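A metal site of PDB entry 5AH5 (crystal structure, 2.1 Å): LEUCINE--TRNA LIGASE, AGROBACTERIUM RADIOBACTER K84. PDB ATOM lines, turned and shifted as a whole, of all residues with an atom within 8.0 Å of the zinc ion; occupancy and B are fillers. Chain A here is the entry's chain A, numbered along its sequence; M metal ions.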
ATOM      1  N   ILE A 430     -24.090 -19.688  19.513  1.00  0.00           N
ATOM      2  CA  ILE A 430     -22.819 -18.991  19.760  1.00  0.00           C
ATOM      3  C   ILE A 430     -21.963 -19.766  20.733  1.00  0.00           C
ATOM      4  O   ILE A 430     -22.466 -20.209  21.781  1.00  0.00           O
ATOM      5  CB  ILE A 430     -23.071 -17.538  20.236  1.00  0.00           C
ATOM      6  CG1 ILE A 430     -23.666 -16.727  19.112  1.00  0.00           C
ATOM      7  CG2 ILE A 430     -21.748 -16.870  20.625  1.00  0.00           C
ATOM      8  CD1 ILE A 430     -24.325 -15.417  19.554  1.00  0.00           C
ATOM      9  N   HIS A 431     -20.679 -19.960  20.389  1.00  0.00           N
ATOM     10  CA  HIS A 431     -19.767 -20.700  21.248  1.00  0.00           C
ATOM     11  C   HIS A 431     -18.892 -19.747  22.104  1.00  0.00           C
ATOM     12  O   HIS A 431     -18.087 -18.984  21.558  1.00  0.00           O
ATOM     13  CB  HIS A 431     -18.849 -21.597  20.425  1.00  0.00           C
ATOM     14  CG  HIS A 431     -19.581 -22.618  19.611  1.00  0.00           C
ATOM     15  ND1 HIS A 431     -19.776 -23.913  20.033  1.00  0.00           N
ATOM     16  CD2 HIS A 431     -20.186 -22.518  18.398  1.00  0.00           C
ATOM     17  CE1 HIS A 431     -20.460 -24.568  19.126  1.00  0.00           C
ATOM     18  NE2 HIS A 431     -20.734 -23.743  18.130  1.00  0.00           N
ATOM     19  N   CYS A 432     -19.085 -19.822  23.424  1.00  0.00           N
ATOM     20  CA  CYS A 432     -18.331 -19.037  24.390  1.00  0.00           C
ATOM     21  C   CYS A 432     -17.306 -19.925  25.118  1.00  0.00           C
ATOM     22  O   CYS A 432     -17.603 -21.086  25.458  1.00  0.00           O
ATOM     23  CB  CYS A 432     -19.271 -18.383  25.396  1.00  0.00           C
ATOM     24  SG  CYS A 432     -18.449 -17.197  26.526  1.00  0.00           S
ATOM     25  N   SER A 433     -16.102 -19.388  25.305  1.00  0.00           N
ATOM     26  CA  SER A 433     -15.055 -20.004  26.155  1.00  0.00           C
ATOM     27  C   SER A 433     -15.548 -20.245  27.570  1.00  0.00           C
ATOM     28  O   SER A 433     -15.273 -21.288  28.167  1.00  0.00           O
ATOM     29  CB  SER A 433     -13.826 -19.093  26.248  1.00  0.00           C
ATOM     30  OG  SER A 433     -13.238 -18.909  24.985  1.00  0.00           O
ATOM     31  N   GLU A 434     -16.277 -19.265  28.092  1.00  0.00           N
ATOM     32  CA  GLU A 434     -16.746 -19.305  29.473  1.00  0.00           C
ATOM     33  C   GLU A 434     -18.005 -20.202  29.541  1.00  0.00           C
ATOM     34  O   GLU A 434     -17.988 -21.304  30.098  1.00  0.00           O
ATOM     35  CB  GLU A 434     -17.005 -17.886  30.025  1.00  0.00           C
ATOM     36  CG  GLU A 434     -15.989 -16.782  29.632  1.00  0.00           C
ATOM     37  CD  GLU A 434     -14.506 -17.150  29.820  1.00  0.00           C
ATOM     38  OE1 GLU A 434     -14.127 -17.626  30.925  1.00  0.00           O
ATOM     39  OE2 GLU A 434     -13.713 -16.960  28.872  1.00  0.00           O
ATOM     40  N   CYS A 435     -19.072 -19.740  28.900  1.00  0.00           N
ATOM     41  CA  CYS A 435     -20.406 -20.315  29.073  1.00  0.00           C
ATOM     42  C   CYS A 435     -20.684 -21.647  28.308  1.00  0.00           C
ATOM     43  O   CYS A 435     -21.558 -22.420  28.713  1.00  0.00           O
ATOM     44  CB  CYS A 435     -21.456 -19.242  28.748  1.00  0.00           C
ATOM     45  SG  CYS A 435     -21.110 -17.575  29.423  1.00  0.00           S
ATOM     46  N   GLY A 436     -19.946 -21.944  27.233  1.00  0.00           N
ATOM     47  CA  GLY A 436     -20.243 -23.104  26.357  1.00  0.00           C
ATOM     48  C   GLY A 436     -21.128 -22.701  25.176  1.00  0.00           C
ATOM     49  O   GLY A 436     -21.033 -21.549  24.687  1.00  0.00           O
ATOM     50  N   ILE A 438     -24.452 -21.566  23.395  1.00  0.00           N
ATOM     51  CA  ILE A 438     -25.472 -20.681  23.870  1.00  0.00           C
ATOM     52  C   ILE A 438     -26.343 -20.382  22.663  1.00  0.00           C
ATOM     53  O   ILE A 438     -25.830 -20.067  21.590  1.00  0.00           O
ATOM     54  CB  ILE A 438     -24.847 -19.371  24.513  1.00  0.00           C
ATOM     55  CG1 ILE A 438     -24.672 -19.500  26.030  1.00  0.00           C
ATOM     56  CG2 ILE A 438     -25.818 -18.192  24.425  1.00  0.00           C
ATOM     57  CD1 ILE A 438     -23.939 -20.677  26.572  1.00  0.00           C
ATOM     58  N   LYS A 472     -21.054 -11.578  20.104  1.00  0.00           N
ATOM     59  CA  LYS A 472     -21.056 -11.368  21.525  1.00  0.00           C
ATOM     60  C   LYS A 472     -21.867 -12.452  22.150  1.00  0.00           C
ATOM     61  O   LYS A 472     -22.930 -12.833  21.651  1.00  0.00           O
ATOM     62  CB  LYS A 472     -21.561  -9.961  21.862  1.00  0.00           C
ATOM     63  CG  LYS A 472     -20.431  -8.933  21.787  1.00  0.00           C
ATOM     64  CD  LYS A 472     -20.858  -7.631  21.120  1.00  0.00           C
ATOM     65  CE  LYS A 472     -19.664  -6.719  20.908  1.00  0.00           C
ATOM     66  NZ  LYS A 472     -20.092  -5.478  20.204  1.00  0.00           N
ATOM     67  N   CYS A 473     -21.336 -12.979  23.222  1.00  0.00           N
ATOM     68  CA  CYS A 473     -22.003 -13.990  23.937  1.00  0.00           C
ATOM     69  C   CYS A 473     -23.314 -13.426  24.561  1.00  0.00           C
ATOM     70  O   CYS A 473     -23.286 -12.437  25.318  1.00  0.00           O
ATOM     71  CB  CYS A 473     -21.068 -14.511  24.985  1.00  0.00           C
ATOM     72  SG  CYS A 473     -21.947 -15.656  26.008  1.00  0.00           S
ATOM     73  N   PRO A 474     -24.482 -14.023  24.214  1.00  0.00           N
ATOM     74  CA  PRO A 474     -25.769 -13.607  24.790  1.00  0.00           C
ATOM     75  C   PRO A 474     -25.873 -13.716  26.317  1.00  0.00           C
ATOM     76  O   PRO A 474     -26.574 -12.899  26.930  1.00  0.00           O
ATOM     77  CB  PRO A 474     -26.789 -14.552  24.103  1.00  0.00           C
ATOM     78  CG  PRO A 474     -26.143 -14.937  22.836  1.00  0.00           C
ATOM     79  CD  PRO A 474     -24.680 -15.054  23.173  1.00  0.00           C
ATOM     80  N   GLN A 475     -25.214 -14.702  26.929  1.00  0.00           N
ATOM     81  CA  GLN A 475     -25.198 -14.812  28.376  1.00  0.00           C
ATOM     82  C   GLN A 475     -24.288 -13.701  28.997  1.00  0.00           C
ATOM     83  O   GLN A 475     -24.804 -12.786  29.644  1.00  0.00           O
ATOM     84  CB  GLN A 475     -24.774 -16.217  28.785  1.00  0.00           C
ATOM     85  CG  GLN A 475     -25.172 -16.638  30.195  1.00  0.00           C
ATOM     86  CD  GLN A 475     -25.453 -18.122  30.267  1.00  0.00           C
ATOM     87  OE1 GLN A 475     -24.535 -18.940  30.268  1.00  0.00           O
ATOM     88  NE2 GLN A 475     -26.724 -18.486  30.299  1.00  0.00           N
ATOM     89  N   CYS A 476     -22.981 -13.757  28.763  1.00  0.00           N
ATOM     90  CA  CYS A 476     -22.038 -12.902  29.512  1.00  0.00           C
ATOM     91  C   CYS A 476     -21.662 -11.580  28.846  1.00  0.00           C
ATOM     92  O   CYS A 476     -21.154 -10.713  29.524  1.00  0.00           O
ATOM     93  CB  CYS A 476     -20.760 -13.670  29.858  1.00  0.00           C
ATOM     94  SG  CYS A 476     -19.595 -13.840  28.488  1.00  0.00           S
ATOM     95  N   GLY A 477     -21.908 -11.423  27.543  1.00  0.00           N
ATOM     96  CA  GLY A 477     -21.447 -10.227  26.764  1.00  0.00           C
ATOM     97  C   GLY A 477     -19.990 -10.237  26.258  1.00  0.00           C
ATOM     98  O   GLY A 477     -19.620  -9.361  25.447  1.00  0.00           O
ATOM     99  N   GLY A 478     -19.174 -11.202  26.710  1.00  0.00           N
ATOM    100  CA  GLY A 478     -17.798 -11.413  26.219  1.00  0.00           C
ATOM    101  C   GLY A 478     -17.683 -11.672  24.721  1.00  0.00           C
ATOM    102  O   GLY A 478     -18.702 -11.830  24.036  1.00  0.00           O
ATOM    103  N   ASP A 479     -16.462 -11.655  24.194  1.00  0.00           N
ATOM    104  CA  ASP A 479     -16.244 -11.965  22.768  1.00  0.00           C
ATOM    105  C   ASP A 479     -16.346 -13.504  22.607  1.00  0.00           C
ATOM    106  O   ASP A 479     -15.787 -14.294  23.400  1.00  0.00           O
ATOM    107  CB  ASP A 479     -14.910 -11.424  22.231  1.00  0.00           C
ATOM    108  CG  ASP A 479     -14.837  -9.864  22.185  1.00  0.00           C
ATOM    109  OD1 ASP A 479     -15.837  -9.183  21.822  1.00  0.00           O
ATOM    110  OD2 ASP A 479     -13.751  -9.324  22.497  1.00  0.00           O
ATOM    111  N   ALA A 480     -17.080 -13.919  21.592  1.00  0.00           N
ATOM    112  CA  ALA A 480     -17.403 -15.329  21.370  1.00  0.00           C
ATOM    113  C   ALA A 480     -17.440 -15.542  19.846  1.00  0.00           C
ATOM    114  O   ALA A 480     -17.027 -14.672  19.088  1.00  0.00           O
ATOM    115  CB  ALA A 480     -18.737 -15.630  22.010  1.00  0.00           C
HETATM  116 ZN    ZN M   1     -20.369 -16.227  27.615  1.00  0.00          ZN
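The side-chain sulfur of Cys 432 sits close to the backbone NH of Glu 434.
The backbone NH (N) of Gly 478 lies close to the side-chain sulfur (SG) of Cys 476, 3.2 Å away.
The backbone carbonyl oxygen (O) of Gly 478 sits at hydrogen-bond distance from the backbone NH (N) of Cys 473, at 3.0 Å.
The side-chain sulfur of Cys 473 sits close to the backbone NH of Gln 475, at 3.5 Å.
The side-chain amide oxygen of Gln 475 sits close to the side-chain sulfur of Cys 435 (3.8 Å).
Of the 17 residues printed, 4 come within 4 Å of the zinc ion.
The zinc ion is bound by the side-chain sulfur (SG) of Cys 473, the side-chain sulfur (SG) of Cys 435, the side-chain sulfur (SG) of Cys 432 and the side-chain sulfur (SG) of Cys 476.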
